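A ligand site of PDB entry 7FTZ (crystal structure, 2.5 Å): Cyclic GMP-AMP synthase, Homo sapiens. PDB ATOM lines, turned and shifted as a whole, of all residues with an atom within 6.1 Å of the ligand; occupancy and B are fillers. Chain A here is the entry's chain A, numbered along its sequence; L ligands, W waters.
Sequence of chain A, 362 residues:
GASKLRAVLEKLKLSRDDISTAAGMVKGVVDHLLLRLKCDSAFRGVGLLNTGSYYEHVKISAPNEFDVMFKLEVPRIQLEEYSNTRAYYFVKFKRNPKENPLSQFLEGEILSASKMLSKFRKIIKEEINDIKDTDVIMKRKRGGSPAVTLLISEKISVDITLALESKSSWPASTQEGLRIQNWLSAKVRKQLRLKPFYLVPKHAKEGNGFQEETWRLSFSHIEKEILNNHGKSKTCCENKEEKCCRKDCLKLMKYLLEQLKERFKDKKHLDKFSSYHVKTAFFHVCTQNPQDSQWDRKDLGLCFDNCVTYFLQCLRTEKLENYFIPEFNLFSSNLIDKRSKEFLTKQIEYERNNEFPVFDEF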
ATOM      1  N   ALA A  87     -15.163  -0.588  11.003  1.00  0.00           N
ATOM      2  CA  ALA A  87     -14.727   0.261  12.104  1.00  0.00           C
ATOM      3  C   ALA A  87     -15.834   0.863  12.943  1.00  0.00           C
ATOM      4  O   ALA A  87     -15.590   1.232  14.099  1.00  0.00           O
ATOM      5  CB  ALA A  87     -13.850   1.373  11.579  1.00  0.00           C
ATOM      6  N   TYR A  88     -17.017   1.032  12.357  1.00  0.00           N
ATOM      7  CA  TYR A  88     -18.143   1.674  13.033  1.00  0.00           C
ATOM      8  C   TYR A  88     -19.154   0.647  13.486  1.00  0.00           C
ATOM      9  O   TYR A  88     -19.492  -0.261  12.737  1.00  0.00           O
ATOM     10  CB  TYR A  88     -18.753   2.780  12.140  1.00  0.00           C
ATOM     11  CG  TYR A  88     -17.781   3.891  11.807  1.00  0.00           C
ATOM     12  CD1 TYR A  88     -16.909   3.783  10.731  1.00  0.00           C
ATOM     13  CD2 TYR A  88     -17.737   5.067  12.568  1.00  0.00           C
ATOM     14  CE1 TYR A  88     -15.998   4.802  10.412  1.00  0.00           C
ATOM     15  CE2 TYR A  88     -16.846   6.105  12.252  1.00  0.00           C
ATOM     16  CZ  TYR A  88     -15.985   5.965  11.164  1.00  0.00           C
ATOM     17  OH  TYR A  88     -15.101   6.972  10.862  1.00  0.00           O
ATOM     18  N   GLY A 143     -18.621  16.963  15.523  1.00  0.00           N
ATOM     19  CA  GLY A 143     -17.651  15.953  15.101  1.00  0.00           C
ATOM     20  C   GLY A 143     -17.625  14.687  15.924  1.00  0.00           C
ATOM     21  O   GLY A 143     -16.863  13.758  15.599  1.00  0.00           O
ATOM     22  N   SER A 145     -16.148  13.267  18.464  1.00  0.00           N
ATOM     23  CA  SER A 145     -14.933  13.244  19.273  1.00  0.00           C
ATOM     24  C   SER A 145     -13.757  13.975  18.577  1.00  0.00           C
ATOM     25  O   SER A 145     -13.528  13.688  17.403  1.00  0.00           O
ATOM     26  CB  SER A 145     -14.554  11.801  19.637  1.00  0.00           C
ATOM     27  OG  SER A 145     -15.276  11.372  20.780  1.00  0.00           O
ATOM     28  N   PRO A 146     -13.021  14.928  19.232  1.00  0.00           N
ATOM     29  CA  PRO A 146     -13.131  15.391  20.639  1.00  0.00           C
ATOM     30  C   PRO A 146     -14.468  16.041  21.019  1.00  0.00           C
ATOM     31  O   PRO A 146     -14.927  17.003  20.394  1.00  0.00           O
ATOM     32  CB  PRO A 146     -11.939  16.366  20.780  1.00  0.00           C
ATOM     33  CG  PRO A 146     -11.631  16.803  19.389  1.00  0.00           C
ATOM     34  CD  PRO A 146     -11.899  15.596  18.537  1.00  0.00           C
ATOM     35  N   LYS A 202     -18.505   8.575  17.081  1.00  0.00           N
ATOM     36  CA  LYS A 202     -18.049   9.024  15.767  1.00  0.00           C
ATOM     37  C   LYS A 202     -19.088   8.786  14.707  1.00  0.00           C
ATOM     38  O   LYS A 202     -19.515   7.653  14.500  1.00  0.00           O
ATOM     39  CB  LYS A 202     -16.707   8.382  15.376  1.00  0.00           C
ATOM     40  CG  LYS A 202     -15.529   9.346  15.433  1.00  0.00           C
ATOM     41  CD  LYS A 202     -15.450  10.222  14.216  1.00  0.00           C
ATOM     42  CE  LYS A 202     -14.699  11.487  14.520  1.00  0.00           C
ATOM     43  NZ  LYS A 202     -15.162  12.613  13.670  1.00  0.00           N
ATOM     44  N   ARG A 216     -16.860   4.314  17.173  1.00  0.00           N
ATOM     45  CA  ARG A 216     -15.682   3.852  16.410  1.00  0.00           C
ATOM     46  C   ARG A 216     -14.621   3.242  17.338  1.00  0.00           C
ATOM     47  O   ARG A 216     -14.507   3.671  18.481  1.00  0.00           O
ATOM     48  CB  ARG A 216     -15.092   5.041  15.630  1.00  0.00           C
ATOM     49  CG  ARG A 216     -14.180   4.707  14.450  1.00  0.00           C
ATOM     50  CD  ARG A 216     -13.220   5.843  14.198  1.00  0.00           C
ATOM     51  NE  ARG A 216     -12.282   5.969  15.321  1.00  0.00           N
ATOM     52  CZ  ARG A 216     -11.765   7.106  15.780  1.00  0.00           C
ATOM     53  NH1 ARG A 216     -12.065   8.264  15.174  1.00  0.00           N
ATOM     54  NH2 ARG A 216     -10.938   7.104  16.806  1.00  0.00           N
ATOM     55  N   LEU A 217     -13.833   2.256  16.839  1.00  0.00           N
ATOM     56  CA  LEU A 217     -12.750   1.642  17.632  1.00  0.00           C
ATOM     57  C   LEU A 217     -11.601   2.646  17.877  1.00  0.00           C
ATOM     58  O   LEU A 217     -11.222   3.416  16.987  1.00  0.00           O
ATOM     59  CB  LEU A 217     -12.205   0.346  16.983  1.00  0.00           C
ATOM     60  CG  LEU A 217     -13.081  -0.909  17.045  1.00  0.00           C
ATOM     61  CD1 LEU A 217     -12.631  -1.943  16.008  1.00  0.00           C
ATOM     62  CD2 LEU A 217     -13.075  -1.541  18.443  1.00  0.00           C
ATOM     63  N   SER A 218     -11.061   2.651  19.105  1.00  0.00           N
ATOM     64  CA  SER A 218      -9.980   3.532  19.559  1.00  0.00           C
ATOM     65  C   SER A 218      -8.786   2.702  20.092  1.00  0.00           C
ATOM     66  O   SER A 218      -8.947   1.874  20.995  1.00  0.00           O
ATOM     67  CB  SER A 218     -10.504   4.514  20.605  1.00  0.00           C
ATOM     68  OG  SER A 218      -9.683   5.660  20.701  1.00  0.00           O
ATOM     69  N   PHE A 219      -7.595   2.901  19.481  1.00  0.00           N
ATOM     70  CA  PHE A 219      -6.371   2.166  19.843  1.00  0.00           C
ATOM     71  C   PHE A 219      -5.215   3.062  20.328  1.00  0.00           C
ATOM     72  O   PHE A 219      -4.037   2.714  20.198  1.00  0.00           O
ATOM     73  CB  PHE A 219      -5.929   1.273  18.677  1.00  0.00           C
ATOM     74  CG  PHE A 219      -6.961   0.293  18.183  1.00  0.00           C
ATOM     75  CD1 PHE A 219      -7.136  -0.942  18.818  1.00  0.00           C
ATOM     76  CD2 PHE A 219      -7.735   0.564  17.061  1.00  0.00           C
ATOM     77  CE1 PHE A 219      -8.079  -1.859  18.352  1.00  0.00           C
ATOM     78  CE2 PHE A 219      -8.659  -0.364  16.588  1.00  0.00           C
ATOM     79  CZ  PHE A 219      -8.823  -1.566  17.234  1.00  0.00           C
ATOM     80  N   SER A 220      -5.573   4.220  20.940  1.00  0.00           N
ATOM     81  CA  SER A 220      -4.660   5.215  21.508  1.00  0.00           C
ATOM     82  C   SER A 220      -3.704   4.617  22.544  1.00  0.00           C
ATOM     83  O   SER A 220      -2.535   4.999  22.579  1.00  0.00           O
ATOM     84  CB  SER A 220      -5.437   6.363  22.115  1.00  0.00           C
ATOM     85  OG  SER A 220      -5.753   7.324  21.132  1.00  0.00           O
ATOM     86  N   GLU A 223      -0.998   2.464  20.703  1.00  0.00           N
ATOM     87  CA  GLU A 223      -0.115   3.374  19.979  1.00  0.00           C
ATOM     88  C   GLU A 223       1.032   3.812  20.891  1.00  0.00           C
ATOM     89  O   GLU A 223       2.196   3.661  20.520  1.00  0.00           O
ATOM     90  CB  GLU A 223      -0.936   4.588  19.509  1.00  0.00           C
ATOM     91  CG  GLU A 223      -0.184   5.542  18.607  1.00  0.00           C
ATOM     92  CD  GLU A 223      -0.571   6.994  18.813  1.00  0.00           C
ATOM     93  OE1 GLU A 223       0.343   7.826  19.036  1.00  0.00           O
ATOM     94  OE2 GLU A 223      -1.783   7.313  18.767  1.00  0.00           O
ATOM     95  N   SER A 274      -4.656  14.240   9.119  1.00  0.00           N
ATOM     96  CA  SER A 274      -4.289  14.392  10.530  1.00  0.00           C
ATOM     97  C   SER A 274      -3.081  13.544  10.885  1.00  0.00           C
ATOM     98  O   SER A 274      -2.620  12.751  10.063  1.00  0.00           O
ATOM     99  CB  SER A 274      -5.481  14.055  11.440  1.00  0.00           C
ATOM    100  OG  SER A 274      -6.002  12.755  11.211  1.00  0.00           O
ATOM    101  N   SER A 275      -2.564  13.691  12.131  1.00  0.00           N
ATOM    102  CA  SER A 275      -1.419  12.944  12.672  1.00  0.00           C
ATOM    103  C   SER A 275      -1.627  11.445  12.648  1.00  0.00           C
ATOM    104  O   SER A 275      -0.666  10.677  12.684  1.00  0.00           O
ATOM    105  CB  SER A 275      -1.128  13.404  14.095  1.00  0.00           C
ATOM    106  OG  SER A 275      -2.225  13.128  14.956  1.00  0.00           O
ATOM    107  N   TYR A 276      -2.892  11.018  12.577  1.00  0.00           N
ATOM    108  CA  TYR A 276      -3.294   9.613  12.553  1.00  0.00           C
ATOM    109  C   TYR A 276      -2.957   8.960  11.235  1.00  0.00           C
ATOM    110  O   TYR A 276      -2.548   7.806  11.237  1.00  0.00           O
ATOM    111  CB  TYR A 276      -4.758   9.468  12.945  1.00  0.00           C
ATOM    112  CG  TYR A 276      -4.978   9.922  14.376  1.00  0.00           C
ATOM    113  CD1 TYR A 276      -4.632   9.108  15.449  1.00  0.00           C
ATOM    114  CD2 TYR A 276      -5.462  11.200  14.658  1.00  0.00           C
ATOM    115  CE1 TYR A 276      -4.811   9.520  16.772  1.00  0.00           C
ATOM    116  CE2 TYR A 276      -5.673  11.620  15.972  1.00  0.00           C
ATOM    117  CZ  TYR A 276      -5.341  10.783  17.029  1.00  0.00           C
ATOM    118  OH  TYR A 276      -5.528  11.201  18.324  1.00  0.00           O
ATOM    119  N   LYS A 279       0.895   8.548  11.637  1.00  0.00           N
ATOM    120  CA  LYS A 279       1.249   7.450  12.557  1.00  0.00           C
ATOM    121  C   LYS A 279       0.942   6.067  11.974  1.00  0.00           C
ATOM    122  O   LYS A 279       1.748   5.154  12.155  1.00  0.00           O
ATOM    123  CB  LYS A 279       0.554   7.589  13.913  1.00  0.00           C
ATOM    124  CG  LYS A 279       0.953   8.780  14.773  1.00  0.00           C
ATOM    125  CD  LYS A 279      -0.183   8.981  15.773  1.00  0.00           C
ATOM    126  CE  LYS A 279      -0.107  10.232  16.616  1.00  0.00           C
ATOM    127  NZ  LYS A 279      -1.449  10.569  17.160  1.00  0.00           N
ATOM    128  N   THR A 280      -0.204   5.927  11.259  1.00  0.00           N
ATOM    129  CA  THR A 280      -0.619   4.686  10.583  1.00  0.00           C
ATOM    130  C   THR A 280       0.438   4.320   9.532  1.00  0.00           C
ATOM    131  O   THR A 280       0.882   3.176   9.513  1.00  0.00           O
ATOM    132  CB  THR A 280      -2.005   4.853   9.928  1.00  0.00           C
ATOM    133  OG1 THR A 280      -2.945   5.109  10.948  1.00  0.00           O
ATOM    134  CG2 THR A 280      -2.450   3.629   9.144  1.00  0.00           C
ATOM    135  N   PHE A 283       3.918   3.183  11.161  1.00  0.00           N
ATOM    136  CA  PHE A 283       3.846   1.828  11.682  1.00  0.00           C
ATOM    137  C   PHE A 283       3.959   0.794  10.565  1.00  0.00           C
ATOM    138  O   PHE A 283       4.530  -0.274  10.803  1.00  0.00           O
ATOM    139  CB  PHE A 283       2.589   1.609  12.542  1.00  0.00           C
ATOM    140  CG  PHE A 283       2.575   2.320  13.880  1.00  0.00           C
ATOM    141  CD1 PHE A 283       3.748   2.463  14.630  1.00  0.00           C
ATOM    142  CD2 PHE A 283       1.394   2.806  14.419  1.00  0.00           C
ATOM    143  CE1 PHE A 283       3.732   3.150  15.852  1.00  0.00           C
ATOM    144  CE2 PHE A 283       1.385   3.466  15.654  1.00  0.00           C
ATOM    145  CZ  PHE A 283       2.545   3.611  16.370  1.00  0.00           C
ATOM    146  N   ASN A 322      -5.665   0.672   7.426  1.00  0.00           N
ATOM    147  CA  ASN A 322      -5.691   0.938   8.852  1.00  0.00           C
ATOM    148  C   ASN A 322      -4.728  -0.099   9.522  1.00  0.00           C
ATOM    149  O   ASN A 322      -4.660  -1.263   9.108  1.00  0.00           O
ATOM    150  CB  ASN A 322      -7.108   0.851   9.401  1.00  0.00           C
ATOM    151  CG  ASN A 322      -7.227   1.267  10.836  1.00  0.00           C
ATOM    152  OD1 ASN A 322      -6.991   0.473  11.761  1.00  0.00           O
ATOM    153  ND2 ASN A 322      -7.602   2.521  11.032  1.00  0.00           N
ATOM    154  N   TYR A 323      -3.933   0.365  10.480  1.00  0.00           N
ATOM    155  CA  TYR A 323      -2.969  -0.507  11.130  1.00  0.00           C
ATOM    156  C   TYR A 323      -3.600  -1.626  11.981  1.00  0.00           C
ATOM    157  O   TYR A 323      -2.989  -2.693  12.155  1.00  0.00           O
ATOM    158  CB  TYR A 323      -1.954   0.317  11.920  1.00  0.00           C
ATOM    159  CG  TYR A 323      -0.664  -0.440  12.154  1.00  0.00           C
ATOM    160  CD1 TYR A 323       0.243  -0.662  11.105  1.00  0.00           C
ATOM    161  CD2 TYR A 323      -0.369  -0.999  13.393  1.00  0.00           C
ATOM    162  CE1 TYR A 323       1.401  -1.420  11.299  1.00  0.00           C
ATOM    163  CE2 TYR A 323       0.805  -1.719  13.605  1.00  0.00           C
ATOM    164  CZ  TYR A 323       1.695  -1.910  12.562  1.00  0.00           C
ATOM    165  OH  TYR A 323       2.849  -2.615  12.794  1.00  0.00           O
ATOM    166  N   PHE A 324      -4.852  -1.397  12.441  1.00  0.00           N
ATOM    167  CA  PHE A 324      -5.605  -2.295  13.318  1.00  0.00           C
ATOM    168  C   PHE A 324      -6.734  -3.059  12.621  1.00  0.00           C
ATOM    169  O   PHE A 324      -6.966  -4.212  12.973  1.00  0.00           O
ATOM    170  CB  PHE A 324      -6.111  -1.514  14.530  1.00  0.00           C
ATOM    171  CG  PHE A 324      -5.016  -0.794  15.273  1.00  0.00           C
ATOM    172  CD1 PHE A 324      -4.226  -1.464  16.215  1.00  0.00           C
ATOM    173  CD2 PHE A 324      -4.754   0.553  15.036  1.00  0.00           C
ATOM    174  CE1 PHE A 324      -3.221  -0.805  16.913  1.00  0.00           C
ATOM    175  CE2 PHE A 324      -3.725   1.210  15.715  1.00  0.00           C
ATOM    176  CZ  PHE A 324      -2.956   0.539  16.646  1.00  0.00           C
ATOM    177  N   ILE A 325      -7.396  -2.432  11.636  1.00  0.00           N
ATOM    178  CA  ILE A 325      -8.515  -2.996  10.826  1.00  0.00           C
ATOM    179  C   ILE A 325      -8.042  -2.998   9.342  1.00  0.00           C
ATOM    180  O   ILE A 325      -8.256  -2.023   8.623  1.00  0.00           O
ATOM    181  CB  ILE A 325      -9.812  -2.165  11.037  1.00  0.00           C
ATOM    182  CG1 ILE A 325     -10.133  -1.943  12.546  1.00  0.00           C
ATOM    183  CG2 ILE A 325     -10.988  -2.793  10.293  1.00  0.00           C
ATOM    184  CD1 ILE A 325     -10.619  -0.555  12.912  1.00  0.00           C
ATOM    185  N   PHE A 328     -10.001  -1.598   6.151  1.00  0.00           N
ATOM    186  CA  PHE A 328     -10.304  -0.172   6.188  1.00  0.00           C
ATOM    187  C   PHE A 328      -9.179   0.644   5.530  1.00  0.00           C
ATOM    188  O   PHE A 328      -8.037   0.622   5.995  1.00  0.00           O
ATOM    189  CB  PHE A 328     -10.532   0.280   7.642  1.00  0.00           C
ATOM    190  CG  PHE A 328     -11.316   1.563   7.810  1.00  0.00           C
ATOM    191  CD1 PHE A 328     -10.698   2.793   7.710  1.00  0.00           C
ATOM    192  CD2 PHE A 328     -12.681   1.522   8.056  1.00  0.00           C
ATOM    193  CE1 PHE A 328     -11.431   3.970   7.824  1.00  0.00           C
ATOM    194  CE2 PHE A 328     -13.417   2.705   8.183  1.00  0.00           C
ATOM    195  CZ  PHE A 328     -12.780   3.925   8.075  1.00  0.00           C
ATOM    196  N   LEU A 330      -7.868   4.340   4.777  1.00  0.00           N
ATOM    197  CA  LEU A 330      -7.818   5.732   5.252  1.00  0.00           C
ATOM    198  C   LEU A 330      -7.839   6.751   4.101  1.00  0.00           C
ATOM    199  O   LEU A 330      -8.339   7.861   4.267  1.00  0.00           O
ATOM    200  CB  LEU A 330      -6.541   5.906   6.118  1.00  0.00           C
ATOM    201  CG  LEU A 330      -6.654   5.748   7.649  1.00  0.00           C
ATOM    202  CD1 LEU A 330      -7.316   4.464   8.080  1.00  0.00           C
ATOM    203  CD2 LEU A 330      -5.324   5.787   8.287  1.00  0.00           C
HETATM  204  C1  LIG L   1     -10.135   5.973  12.161  1.00  0.00           C
HETATM  205  C2  LIG L   1      -9.954   3.748  13.289  1.00  0.00           C
HETATM  206  C3  LIG L   1     -11.358   4.032  11.301  1.00  0.00           C
HETATM  207  C4  LIG L   1     -11.015   5.403  11.202  1.00  0.00           C
HETATM  208  C5  LIG L   1      -9.407   2.817  14.359  1.00  0.00           C
HETATM  209  C6  LIG L   1      -7.037   3.679  14.674  1.00  0.00           C
HETATM  210  C7  LIG L   1      -6.056   4.395  15.498  1.00  0.00           C
HETATM  211  C8  LIG L   1      -6.396   4.924  16.777  1.00  0.00           C
HETATM  212  C9  LIG L   1      -5.413   5.615  17.574  1.00  0.00           C
HETATM  213  C10 LIG L   1      -4.102   5.743  17.097  1.00  0.00           C
HETATM  214  C11 LIG L   1      -3.802   5.199  15.833  1.00  0.00           C
HETATM  215  C12 LIG L   1      -4.741   4.556  15.038  1.00  0.00           C
HETATM  216  C13 LIG L   1      -9.610   5.139  13.206  1.00  0.00           C
HETATM  217  C14 LIG L   1     -10.836   3.209  12.324  1.00  0.00           C
HETATM  218  C15 LIG L   1      -9.308   8.237  12.972  1.00  0.00           C
HETATM  219  C16 LIG L   1      -8.983  10.277  13.812  1.00  0.00           C
HETATM  220  C17 LIG L   1      -8.452   9.568  14.849  1.00  0.00           C
HETATM  221  C18 LIG L   1      -9.154  11.771  13.749  1.00  0.00           C
HETATM  222  C19 LIG L   1     -10.642  12.069  14.023  1.00  0.00           C
HETATM  223  N1  LIG L   1      -9.735   7.339  12.020  1.00  0.00           N
HETATM  224  N2  LIG L   1      -8.355   3.504  15.131  1.00  0.00           N
HETATM  225  N3  LIG L   1      -9.475   9.534  12.723  1.00  0.00           N
HETATM  226  O1  LIG L   1      -7.572   4.796  17.383  1.00  0.00           O
HETATM  227  O2  LIG L   1      -6.628   3.210  13.562  1.00  0.00           O
HETATM  228  O3  LIG L   1     -11.476  12.525  13.232  1.00  0.00           O
HETATM  229  O4  LIG L   1     -11.026  11.726  15.303  1.00  0.00           O
HETATM  230  S1  LIG L   1      -8.518   7.893  14.555  1.00  0.00           S
HETATM  231 BR1  LIG L   1      -2.006   5.333  15.114  1.00  0.00          BR
HETATM  232  O   HOH W   1      -8.698   7.531  18.962  1.00  0.00           O
HETATM  233  O   HOH W   2      -4.298   3.008  11.829  1.00  0.00           O
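Residues that only touch the ligand: Ala 87 (3.6 Å), Ser 145 (3.8 Å), Ser 218 (3.5 Å), Ser 220 (3.6 Å), Glu 223 (3.3 Å), Tyr 276 (3.4 Å), Lys 279 (3.6 Å), Phe 283 (3.9 Å), Phe 324 (3.6 Å), Ile 325 (3.8 Å) and Phe 328 (3.5 Å).
Hydrophobic or aromatic side chains that line the ligand: Ala 87, Phe 219, Tyr 276, Phe 283, Phe 324, Ile 325 and Phe 328.
Within 4 Å of the ligand: Ala 87, Ser 145, Lys 202, Arg 216, Leu 217, Ser 218, Phe 219, Ser 220, Glu 223, Tyr 276, Lys 279, Phe 283, Asn 322, Phe 324, Ile 325 and Phe 328.
The nearest printed residue that does not touch the ligand is Ser 274 (4.2 Å).
Water W2 lies within hydrogen-bond range of OG1 of Thr 280, O2 of the ligand, N of Tyr 323 and ND2 of Asn 322.
Water W1 lies within hydrogen-bond range of OG of Ser 218 (2.7 Å), NH2 of Arg 216 (3.1 Å) and O1 of the ligand (3.4 Å).
The backbone NH of Asn 322 is in hydrogen-bond range of the backbone carbonyl oxygen of Phe 328 (2.8 Å).
The side-chain carboxylate of Glu 223 is in salt-bridge range of the side-chain amino group of Lys 279 (3.6 Å).
OG1 of Thr 280 is in hydrogen-bond range of O of Tyr 276, 2.7 Å away.
NZ of Lys 202 lies within hydrogen-bond range of O of Gly 143 (2.8 Å).
The side-chain amino group (NZ) of Lys 279 is in hydrogen-bond range of the side-chain hydroxyl (OG) of Ser 275 (3.5 Å).
N of Leu 217 is in hydrogen-bond range of O of Ala 87 (3.4 Å).
The backbone NH of Phe 324 lies within hydrogen-bond range of the side-chain amide oxygen of Asn 322 (2.9 Å).
OD1 of Asn 322 lies within hydrogen-bond range of N of Ile 325 (2.9 Å).
The guanidinium group of Arg 216 lies within salt-bridge range of an oxygen (O4) of the ligand (3.6 Å).
The backbone NH (N) of Phe 219 sits at hydrogen-bond distance from an oxygen (O1) of the ligand, 2.8 Å away.
NZ of Lys 202 is in salt-bridge range of O3 of the ligand (3.7 Å).
ND2 of Asn 322 sits at hydrogen-bond distance from O2 of the ligand (2.8 Å).
O of Leu 217 sits close to N2 of the ligand (3.4 Å).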
